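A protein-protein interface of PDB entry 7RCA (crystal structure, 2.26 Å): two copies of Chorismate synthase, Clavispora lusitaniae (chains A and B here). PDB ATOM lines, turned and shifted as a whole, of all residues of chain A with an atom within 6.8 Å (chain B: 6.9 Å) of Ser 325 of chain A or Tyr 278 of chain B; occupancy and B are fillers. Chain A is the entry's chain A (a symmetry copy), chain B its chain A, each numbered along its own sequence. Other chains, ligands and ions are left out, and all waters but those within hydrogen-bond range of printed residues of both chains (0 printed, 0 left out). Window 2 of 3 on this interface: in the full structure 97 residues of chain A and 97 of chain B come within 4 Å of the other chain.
Tyr 101 of chain A touches none of the printed residues of chain B.
Ser 325 of chain A touches two residues of chain B.
Of the printed residues of chain B, Thr 326 of chain A touches Leu 286.
Of chain A, only Ser 325 comes within 4 Å of Tyr 278 of chain B.
Printed residues of chain A within 4 Å of Leu 286 of chain B: Thr 326.
Of the printed residues of chain A, Lys 289 of chain B touches Glu 323 (3.97 Å).
The nearest residue of chain A that does not touch Tyr 278 of chain B is Asp 331 of chain A (5.2 Å).
The nearest printed residue of chain B that does not touch Pro 102 of chain A is Leu 286 of chain B (4.3 Å).
Hydrophobic or aromatic side chains of chain B that line the printed part of chain A: Pro 276, Phe 277 and Leu 286.
Along chain B the printed residues that touch a printed residue of chain A span positions 276 to 289.
Hydrophobic or aromatic side chains of chain A that line the printed part of chain B: Pro 102.
Along chain A the printed residues that touch a printed residue of chain B span positions 102 to 326.
Among the printed residues, no Asp or Glu carboxylate lies within 4 Å of a Lys or Arg side-chain nitrogen of the other chain.
Phe 277 of chain B touches Pro 102 of chain A.
O of Glu 323 of chain A touches CB of Pro 276 of chain B, 3.4 Å away.
Glu 323 of chain A touches Lys 289 of chain B.
Thr 324 of chain A touches Phe 277 of chain B (CG2 to N, 3.2 Å).
OG of Ser 325 of chain A touches CA of Tyr 278 of chain B (3.3 Å).
Thr 326 of chain A touches Leu 286 of chain B.
The side-chain hydroxyl (OG) of Ser 325 of chain A lies within hydrogen-bond range of the side-chain carboxylate (OD1) of Asp 331 of chain A.
The side-chain hydroxyl (OG1) of Thr 326 of chain A is in hydrogen-bond range of the backbone NH (N) of Lys 330 of chain A, at 2.7 Å.
The side-chain hydroxyl (OG1) of Thr 326 of chain A sits at hydrogen-bond distance from the backbone NH (N) of Gly 329 of chain A.
The side-chain hydroxyl (OG1) of Thr 326 of chain A lies close to the backbone NH (N) of Asp 328 of chain A.
The backbone carbonyl oxygen (O) of Tyr 278 of chain B is in hydrogen-bond range of the backbone NH (N) of Arg 287 of chain B, at 2.6 Å.
The backbone NH of Lys 289 of chain B sits at hydrogen-bond distance from the backbone carbonyl oxygen of Pro 276 of chain B, at 2.7 Å.
The backbone carbonyl oxygen of Phe 277 of chain B lies within hydrogen-bond range of the side-chain hydroxyl of Ser 325 of chain A.
No position is printed for both chains.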
ATOM      1  N   LEU A 100     -24.487 -16.583  17.538  1.00  0.00           N
ATOM      2  CA  LEU A 100     -23.348 -17.081  18.298  1.00  0.00           C
ATOM      3  C   LEU A 100     -22.187 -16.096  18.234  1.00  0.00           C
ATOM      4  O   LEU A 100     -21.647 -15.699  19.271  1.00  0.00           O
ATOM      5  CB  LEU A 100     -22.919 -18.461  17.790  1.00  0.00           C
ATOM      6  CG  LEU A 100     -23.204 -19.625  18.749  1.00  0.00           C
ATOM      7  CD1 LEU A 100     -22.491 -20.896  18.310  1.00  0.00           C
ATOM      8  CD2 LEU A 100     -22.823 -19.259  20.179  1.00  0.00           C
ATOM      9  N   TYR A 101     -21.810 -15.677  17.027  1.00  0.00           N
ATOM     10  CA  TYR A 101     -20.826 -14.630  16.827  1.00  0.00           C
ATOM     11  C   TYR A 101     -21.480 -13.410  16.195  1.00  0.00           C
ATOM     12  O   TYR A 101     -22.370 -13.556  15.349  1.00  0.00           O
ATOM     13  CB  TYR A 101     -19.671 -15.077  15.920  1.00  0.00           C
ATOM     14  CG  TYR A 101     -19.084 -16.443  16.202  1.00  0.00           C
ATOM     15  CD1 TYR A 101     -19.761 -17.605  15.848  1.00  0.00           C
ATOM     16  CD2 TYR A 101     -17.836 -16.569  16.797  1.00  0.00           C
ATOM     17  CE1 TYR A 101     -19.219 -18.852  16.097  1.00  0.00           C
ATOM     18  CE2 TYR A 101     -17.286 -17.811  17.048  1.00  0.00           C
ATOM     19  CZ  TYR A 101     -17.981 -18.947  16.697  1.00  0.00           C
ATOM     20  OH  TYR A 101     -17.435 -20.184  16.947  1.00  0.00           O
ATOM     21  N   PRO A 102     -21.075 -12.201  16.579  1.00  0.00           N
ATOM     22  CA  PRO A 102     -21.389 -11.033  15.748  1.00  0.00           C
ATOM     23  C   PRO A 102     -20.532 -11.062  14.492  1.00  0.00           C
ATOM     24  O   PRO A 102     -19.309 -11.215  14.564  1.00  0.00           O
ATOM     25  CB  PRO A 102     -21.045  -9.844  16.650  1.00  0.00           C
ATOM     26  CG  PRO A 102     -20.024 -10.377  17.598  1.00  0.00           C
ATOM     27  CD  PRO A 102     -20.365 -11.830  17.816  1.00  0.00           C
ATOM     28  N   GLU A 323     -12.279 -16.453  11.640  1.00  0.00           N
ATOM     29  CA  GLU A 323     -11.988 -16.688  13.050  1.00  0.00           C
ATOM     30  C   GLU A 323     -12.433 -15.463  13.839  1.00  0.00           C
ATOM     31  O   GLU A 323     -11.855 -14.381  13.697  1.00  0.00           O
ATOM     32  CB  GLU A 323     -10.502 -16.966  13.261  1.00  0.00           C
ATOM     33  CG  GLU A 323      -9.953 -18.101  12.417  1.00  0.00           C
ATOM     34  CD  GLU A 323      -8.460 -18.286  12.604  1.00  0.00           C
ATOM     35  OE1 GLU A 323      -7.958 -19.398  12.337  1.00  0.00           O
ATOM     36  OE2 GLU A 323      -7.789 -17.316  13.022  1.00  0.00           O
ATOM     37  N   THR A 324     -13.462 -15.632  14.667  1.00  0.00           N
ATOM     38  CA  THR A 324     -14.046 -14.533  15.419  1.00  0.00           C
ATOM     39  C   THR A 324     -14.444 -15.028  16.801  1.00  0.00           C
ATOM     40  O   THR A 324     -14.607 -16.229  17.031  1.00  0.00           O
ATOM     41  CB  THR A 324     -15.266 -13.943  14.694  1.00  0.00           C
ATOM     42  OG1 THR A 324     -15.062 -14.011  13.278  1.00  0.00           O
ATOM     43  CG2 THR A 324     -15.482 -12.493  15.090  1.00  0.00           C
ATOM     44  N   SER A 325     -14.593 -14.085  17.727  1.00  0.00           N
ATOM     45  CA  SER A 325     -15.047 -14.391  19.075  1.00  0.00           C
ATOM     46  C   SER A 325     -16.558 -14.224  19.175  1.00  0.00           C
ATOM     47  O   SER A 325     -17.164 -13.409  18.474  1.00  0.00           O
ATOM     48  CB  SER A 325     -14.349 -13.496  20.101  1.00  0.00           C
ATOM     49  OG  SER A 325     -12.981 -13.843  20.233  1.00  0.00           O
ATOM     50  N   THR A 326     -17.163 -15.011  20.062  1.00  0.00           N
ATOM     51  CA  THR A 326     -18.610 -15.020  20.223  1.00  0.00           C
ATOM     52  C   THR A 326     -19.074 -13.772  20.973  1.00  0.00           C
ATOM     53  O   THR A 326     -18.283 -12.909  21.365  1.00  0.00           O
ATOM     54  CB  THR A 326     -19.050 -16.277  20.971  1.00  0.00           C
ATOM     55  OG1 THR A 326     -18.298 -16.400  22.186  1.00  0.00           O
ATOM     56  CG2 THR A 326     -18.831 -17.515  20.120  1.00  0.00           C
ATOM     57  N   TYR A 327     -20.394 -13.669  21.161  1.00  0.00           N
ATOM     58  CA  TYR A 327     -20.918 -12.729  22.147  1.00  0.00           C
ATOM     59  C   TYR A 327     -20.497 -13.143  23.548  1.00  0.00           C
ATOM     60  O   TYR A 327     -20.068 -12.305  24.351  1.00  0.00           O
ATOM     61  CB  TYR A 327     -22.440 -12.645  22.052  1.00  0.00           C
ATOM     62  CG  TYR A 327     -22.957 -12.025  20.775  1.00  0.00           C
ATOM     63  CD1 TYR A 327     -22.900 -10.652  20.574  1.00  0.00           C
ATOM     64  CD2 TYR A 327     -23.516 -12.811  19.776  1.00  0.00           C
ATOM     65  CE1 TYR A 327     -23.378 -10.079  19.411  1.00  0.00           C
ATOM     66  CE2 TYR A 327     -23.996 -12.247  18.608  1.00  0.00           C
ATOM     67  CZ  TYR A 327     -23.924 -10.881  18.432  1.00  0.00           C
ATOM     68  OH  TYR A 327     -24.401 -10.314  17.274  1.00  0.00           O
ATOM     69  N   ASP A 328     -20.606 -14.439  23.856  1.00  0.00           N
ATOM     70  CA  ASP A 328     -19.965 -15.008  25.034  1.00  0.00           C
ATOM     71  C   ASP A 328     -18.453 -14.840  24.998  1.00  0.00           C
ATOM     72  O   ASP A 328     -17.791 -15.079  26.017  1.00  0.00           O
ATOM     73  CB  ASP A 328     -20.330 -16.491  25.154  1.00  0.00           C
ATOM     74  CG  ASP A 328     -20.014 -17.063  26.524  1.00  0.00           C
ATOM     75  OD1 ASP A 328     -20.195 -16.340  27.528  1.00  0.00           O
ATOM     76  OD2 ASP A 328     -19.592 -18.237  26.597  1.00  0.00           O
ATOM     77  N   GLY A 329     -17.902 -14.463  23.838  1.00  0.00           N
ATOM     78  CA  GLY A 329     -16.505 -14.067  23.672  1.00  0.00           C
ATOM     79  C   GLY A 329     -15.545 -15.235  23.851  1.00  0.00           C
ATOM     80  O   GLY A 329     -14.630 -15.181  24.680  1.00  0.00           O
ATOM     81  N   LYS A 330     -15.738 -16.289  23.068  1.00  0.00           N
ATOM     82  CA  LYS A 330     -14.790 -17.385  22.988  1.00  0.00           C
ATOM     83  C   LYS A 330     -14.378 -17.564  21.537  1.00  0.00           C
ATOM     84  O   LYS A 330     -15.208 -17.461  20.626  1.00  0.00           O
ATOM     85  CB  LYS A 330     -15.392 -18.685  23.544  1.00  0.00           C
ATOM     86  CG  LYS A 330     -15.937 -18.568  24.968  1.00  0.00           C
ATOM     87  CD  LYS A 330     -14.870 -18.331  26.048  1.00  0.00           C
ATOM     88  CE  LYS A 330     -13.496 -18.901  25.693  1.00  0.00           C
ATOM     89  NZ  LYS A 330     -12.410 -18.264  26.486  1.00  0.00           N
ATOM     90  N   ASP A 331     -13.089 -17.813  21.324  1.00  0.00           N
ATOM     91  CA  ASP A 331     -12.562 -17.909  19.970  1.00  0.00           C
ATOM     92  C   ASP A 331     -13.169 -19.101  19.242  1.00  0.00           C
ATOM     93  O   ASP A 331     -13.228 -20.213  19.777  1.00  0.00           O
ATOM     94  CB  ASP A 331     -11.038 -18.019  20.008  1.00  0.00           C
ATOM     95  CG  ASP A 331     -10.368 -16.709  20.386  1.00  0.00           C
ATOM     96  OD1 ASP A 331     -11.056 -15.820  20.932  1.00  0.00           O
ATOM     97  OD2 ASP A 331      -9.149 -16.571  20.147  1.00  0.00           O
ATOM     98  N   GLY A 332     -13.631 -18.863  18.021  1.00  0.00           N
ATOM     99  CA  GLY A 332     -14.236 -19.908  17.228  1.00  0.00           C
ATOM    100  C   GLY A 332     -14.189 -19.568  15.756  1.00  0.00           C
ATOM    101  O   GLY A 332     -13.592 -18.571  15.346  1.00  0.00           O
ATOM    102  N   PRO B 276     -12.109  -8.876  12.870  1.00  0.00           N
ATOM    103  CA  PRO B 276     -12.597  -9.914  13.786  1.00  0.00           C
ATOM    104  C   PRO B 276     -12.710  -9.390  15.209  1.00  0.00           C
ATOM    105  O   PRO B 276     -12.015  -8.454  15.610  1.00  0.00           O
ATOM    106  CB  PRO B 276     -11.530 -11.014  13.685  1.00  0.00           C
ATOM    107  CG  PRO B 276     -10.684 -10.657  12.492  1.00  0.00           C
ATOM    108  CD  PRO B 276     -10.758  -9.170  12.371  1.00  0.00           C
ATOM    109  N   PHE B 277     -13.601 -10.014  15.975  1.00  0.00           N
ATOM    110  CA  PHE B 277     -13.823  -9.653  17.367  1.00  0.00           C
ATOM    111  C   PHE B 277     -12.957 -10.503  18.294  1.00  0.00           C
ATOM    112  O   PHE B 277     -12.490 -11.584  17.934  1.00  0.00           O
ATOM    113  CB  PHE B 277     -15.299  -9.817  17.744  1.00  0.00           C
ATOM    114  CG  PHE B 277     -16.227  -8.894  17.003  1.00  0.00           C
ATOM    115  CD1 PHE B 277     -16.493  -7.621  17.487  1.00  0.00           C
ATOM    116  CD2 PHE B 277     -16.845  -9.301  15.832  1.00  0.00           C
ATOM    117  CE1 PHE B 277     -17.351  -6.771  16.812  1.00  0.00           C
ATOM    118  CE2 PHE B 277     -17.703  -8.455  15.152  1.00  0.00           C
ATOM    119  CZ  PHE B 277     -17.956  -7.188  15.642  1.00  0.00           C
ATOM    120  N   TYR B 278     -12.757  -9.996  19.509  1.00  0.00           N
ATOM    121  CA  TYR B 278     -11.977 -10.667  20.540  1.00  0.00           C
ATOM    122  C   TYR B 278     -12.223  -9.952  21.863  1.00  0.00           C
ATOM    123  O   TYR B 278     -12.466  -8.743  21.886  1.00  0.00           O
ATOM    124  CB  TYR B 278     -10.480 -10.678  20.186  1.00  0.00           C
ATOM    125  CG  TYR B 278      -9.703  -9.472  20.676  1.00  0.00           C
ATOM    126  CD1 TYR B 278      -9.566  -8.343  19.879  1.00  0.00           C
ATOM    127  CD2 TYR B 278      -9.061  -9.484  21.908  1.00  0.00           C
ATOM    128  CE1 TYR B 278      -8.850  -7.242  20.318  1.00  0.00           C
ATOM    129  CE2 TYR B 278      -8.344  -8.392  22.353  1.00  0.00           C
ATOM    130  CZ  TYR B 278      -8.240  -7.273  21.551  1.00  0.00           C
ATOM    131  OH  TYR B 278      -7.521  -6.185  21.991  1.00  0.00           O
ATOM    132  N   PHE B 279     -12.172 -10.708  22.957  1.00  0.00           N
ATOM    133  CA  PHE B 279     -12.364 -10.127  24.280  1.00  0.00           C
ATOM    134  C   PHE B 279     -11.082  -9.434  24.728  1.00  0.00           C
ATOM    135  O   PHE B 279     -10.001 -10.031  24.699  1.00  0.00           O
ATOM    136  CB  PHE B 279     -12.783 -11.198  25.289  1.00  0.00           C
ATOM    137  CG  PHE B 279     -13.500 -10.649  26.497  1.00  0.00           C
ATOM    138  CD1 PHE B 279     -12.816  -9.958  27.477  1.00  0.00           C
ATOM    139  CD2 PHE B 279     -14.865 -10.798  26.636  1.00  0.00           C
ATOM    140  CE1 PHE B 279     -13.487  -9.460  28.572  1.00  0.00           C
ATOM    141  CE2 PHE B 279     -15.536 -10.298  27.730  1.00  0.00           C
ATOM    142  CZ  PHE B 279     -14.844  -9.625  28.698  1.00  0.00           C
ATOM    143  N   SER B 280     -11.220  -8.179  25.161  1.00  0.00           N
ATOM    144  CA  SER B 280     -10.073  -7.314  25.418  1.00  0.00           C
ATOM    145  C   SER B 280      -9.087  -7.963  26.381  1.00  0.00           C
ATOM    146  O   SER B 280      -9.454  -8.781  27.227  1.00  0.00           O
ATOM    147  CB  SER B 280     -10.543  -5.971  25.984  1.00  0.00           C
ATOM    148  OG  SER B 280      -9.444  -5.201  26.443  1.00  0.00           O
ATOM    149  N   GLU B 281      -7.814  -7.581  26.239  1.00  0.00           N
ATOM    150  CA  GLU B 281      -6.768  -8.150  27.085  1.00  0.00           C
ATOM    151  C   GLU B 281      -6.886  -7.670  28.524  1.00  0.00           C
ATOM    152  O   GLU B 281      -6.482  -8.386  29.448  1.00  0.00           O
ATOM    153  CB  GLU B 281      -5.390  -7.803  26.520  1.00  0.00           C
ATOM    154  CG  GLU B 281      -5.130  -8.339  25.114  1.00  0.00           C
ATOM    155  CD  GLU B 281      -5.528  -9.797  24.944  1.00  0.00           C
ATOM    156  OE1 GLU B 281      -6.064 -10.142  23.870  1.00  0.00           O
ATOM    157  OE2 GLU B 281      -5.278 -10.606  25.864  1.00  0.00           O
ATOM    158  N   GLU B 282      -7.424  -6.469  28.738  1.00  0.00           N
ATOM    159  CA  GLU B 282      -7.760  -6.041  30.092  1.00  0.00           C
ATOM    160  C   GLU B 282      -8.973  -6.781  30.641  1.00  0.00           C
ATOM    161  O   GLU B 282      -9.260  -6.669  31.840  1.00  0.00           O
ATOM    162  CB  GLU B 282      -7.999  -4.530  30.118  1.00  0.00           C
ATOM    163  CG  GLU B 282      -7.902  -3.898  31.502  1.00  0.00           C
ATOM    164  CD  GLU B 282      -6.471  -3.770  31.983  1.00  0.00           C
ATOM    165  OE1 GLU B 282      -5.841  -2.727  31.709  1.00  0.00           O
ATOM    166  OE2 GLU B 282      -5.978  -4.711  32.640  1.00  0.00           O
ATOM    167  N   ARG B 285     -14.464  -6.270  28.039  1.00  0.00           N
ATOM    168  CA  ARG B 285     -15.326  -5.935  26.916  1.00  0.00           C
ATOM    169  C   ARG B 285     -14.866  -6.680  25.671  1.00  0.00           C
ATOM    170  O   ARG B 285     -13.723  -7.134  25.578  1.00  0.00           O
ATOM    171  CB  ARG B 285     -15.331  -4.423  26.669  1.00  0.00           C
ATOM    172  CG  ARG B 285     -16.559  -3.901  25.942  1.00  0.00           C
ATOM    173  CD  ARG B 285     -16.308  -2.494  25.433  1.00  0.00           C
ATOM    174  NE  ARG B 285     -15.886  -2.480  24.038  1.00  0.00           N
ATOM    175  CZ  ARG B 285     -14.852  -1.793  23.574  1.00  0.00           C
ATOM    176  NH1 ARG B 285     -14.089  -1.070  24.377  1.00  0.00           N
ATOM    177  NH2 ARG B 285     -14.574  -1.836  22.275  1.00  0.00           N
ATOM    178  N   LEU B 286     -15.788  -6.799  24.717  1.00  0.00           N
ATOM    179  CA  LEU B 286     -15.481  -7.340  23.399  1.00  0.00           C
ATOM    180  C   LEU B 286     -14.927  -6.230  22.515  1.00  0.00           C
ATOM    181  O   LEU B 286     -15.598  -5.215  22.292  1.00  0.00           O
ATOM    182  CB  LEU B 286     -16.729  -7.953  22.768  1.00  0.00           C
ATOM    183  CG  LEU B 286     -16.517  -9.077  21.747  1.00  0.00           C
ATOM    184  CD1 LEU B 286     -15.631 -10.169  22.317  1.00  0.00           C
ATOM    185  CD2 LEU B 286     -17.839  -9.652  21.257  1.00  0.00           C
ATOM    186  N   ARG B 287     -13.709  -6.416  22.023  1.00  0.00           N
ATOM    187  CA  ARG B 287     -13.044  -5.472  21.137  1.00  0.00           C
ATOM    188  C   ARG B 287     -12.865  -6.111  19.760  1.00  0.00           C
ATOM    189  O   ARG B 287     -13.302  -7.237  19.510  1.00  0.00           O
ATOM    190  CB  ARG B 287     -11.703  -5.042  21.736  1.00  0.00           C
ATOM    191  CG  ARG B 287     -11.796  -3.852  22.685  1.00  0.00           C
ATOM    192  CD  ARG B 287     -10.418  -3.400  23.142  1.00  0.00           C
ATOM    193  NE  ARG B 287      -9.956  -2.226  22.411  1.00  0.00           N
ATOM    194  CZ  ARG B 287      -9.136  -1.309  22.905  1.00  0.00           C
ATOM    195  NH1 ARG B 287      -8.669  -1.394  24.141  1.00  0.00           N
ATOM    196  NH2 ARG B 287      -8.776  -0.280  22.143  1.00  0.00           N
ATOM    197  N   THR B 288     -12.212  -5.380  18.860  1.00  0.00           N
ATOM    198  CA  THR B 288     -11.906  -5.875  17.526  1.00  0.00           C
ATOM    199  C   THR B 288     -10.398  -6.014  17.356  1.00  0.00           C
ATOM    200  O   THR B 288      -9.625  -5.212  17.889  1.00  0.00           O
ATOM    201  CB  THR B 288     -12.461  -4.948  16.436  1.00  0.00           C
ATOM    202  OG1 THR B 288     -12.094  -3.594  16.720  1.00  0.00           O
ATOM    203  CG2 THR B 288     -13.977  -5.054  16.366  1.00  0.00           C
ATOM    204  N   LYS B 289      -9.986  -7.040  16.605  1.00  0.00           N
ATOM    205  CA  LYS B 289      -8.562  -7.263  16.364  1.00  0.00           C
ATOM    206  C   LYS B 289      -7.965  -6.141  15.523  1.00  0.00           C
ATOM    207  O   LYS B 289      -6.941  -5.552  15.889  1.00  0.00           O
ATOM    208  CB  LYS B 289      -8.350  -8.617  15.688  1.00  0.00           C
ATOM    209  CG  LYS B 289      -7.439  -9.558  16.455  1.00  0.00           C
ATOM    210  CD  LYS B 289      -7.559 -10.986  15.943  1.00  0.00           C
ATOM    211  CE  LYS B 289      -8.505 -11.805  16.808  1.00  0.00           C
ATOM    212  NZ  LYS B 289      -9.003 -13.016  16.101  1.00  0.00           N
ATOM    213  N   THR B 290      -8.588  -5.842  14.388  1.00  0.00           N
ATOM    214  CA  THR B 290      -8.207  -4.728  13.533  1.00  0.00           C
ATOM    215  C   THR B 290      -9.307  -3.674  13.557  1.00  0.00           C
ATOM    216  O   THR B 290     -10.434  -3.934  13.994  1.00  0.00           O
ATOM    217  CB  THR B 290      -7.949  -5.193  12.094  1.00  0.00           C
ATOM    218  OG1 THR B 290      -9.079  -5.940  11.618  1.00  0.00           O
ATOM    219  CG2 THR B 290      -6.707  -6.075  12.032  1.00  0.00           C
ATOM    220  N   GLU B 304     -13.898   1.539  19.559  1.00  0.00           N
ATOM    221  CA  GLU B 304     -12.553   1.555  19.010  1.00  0.00           C
ATOM    222  C   GLU B 304     -12.169   2.969  18.581  1.00  0.00           C
ATOM    223  O   GLU B 304     -12.984   3.896  18.589  1.00  0.00           O
ATOM    224  CB  GLU B 304     -12.441   0.595  17.825  1.00  0.00           C
ATOM    225  CG  GLU B 304     -12.737  -0.850  18.171  1.00  0.00           C
ATOM    226  CD  GLU B 304     -11.685  -1.459  19.073  1.00  0.00           C
ATOM    227  OE1 GLU B 304     -12.055  -2.217  19.992  1.00  0.00           O
ATOM    228  OE2 GLU B 304     -10.486  -1.178  18.864  1.00  0.00           O
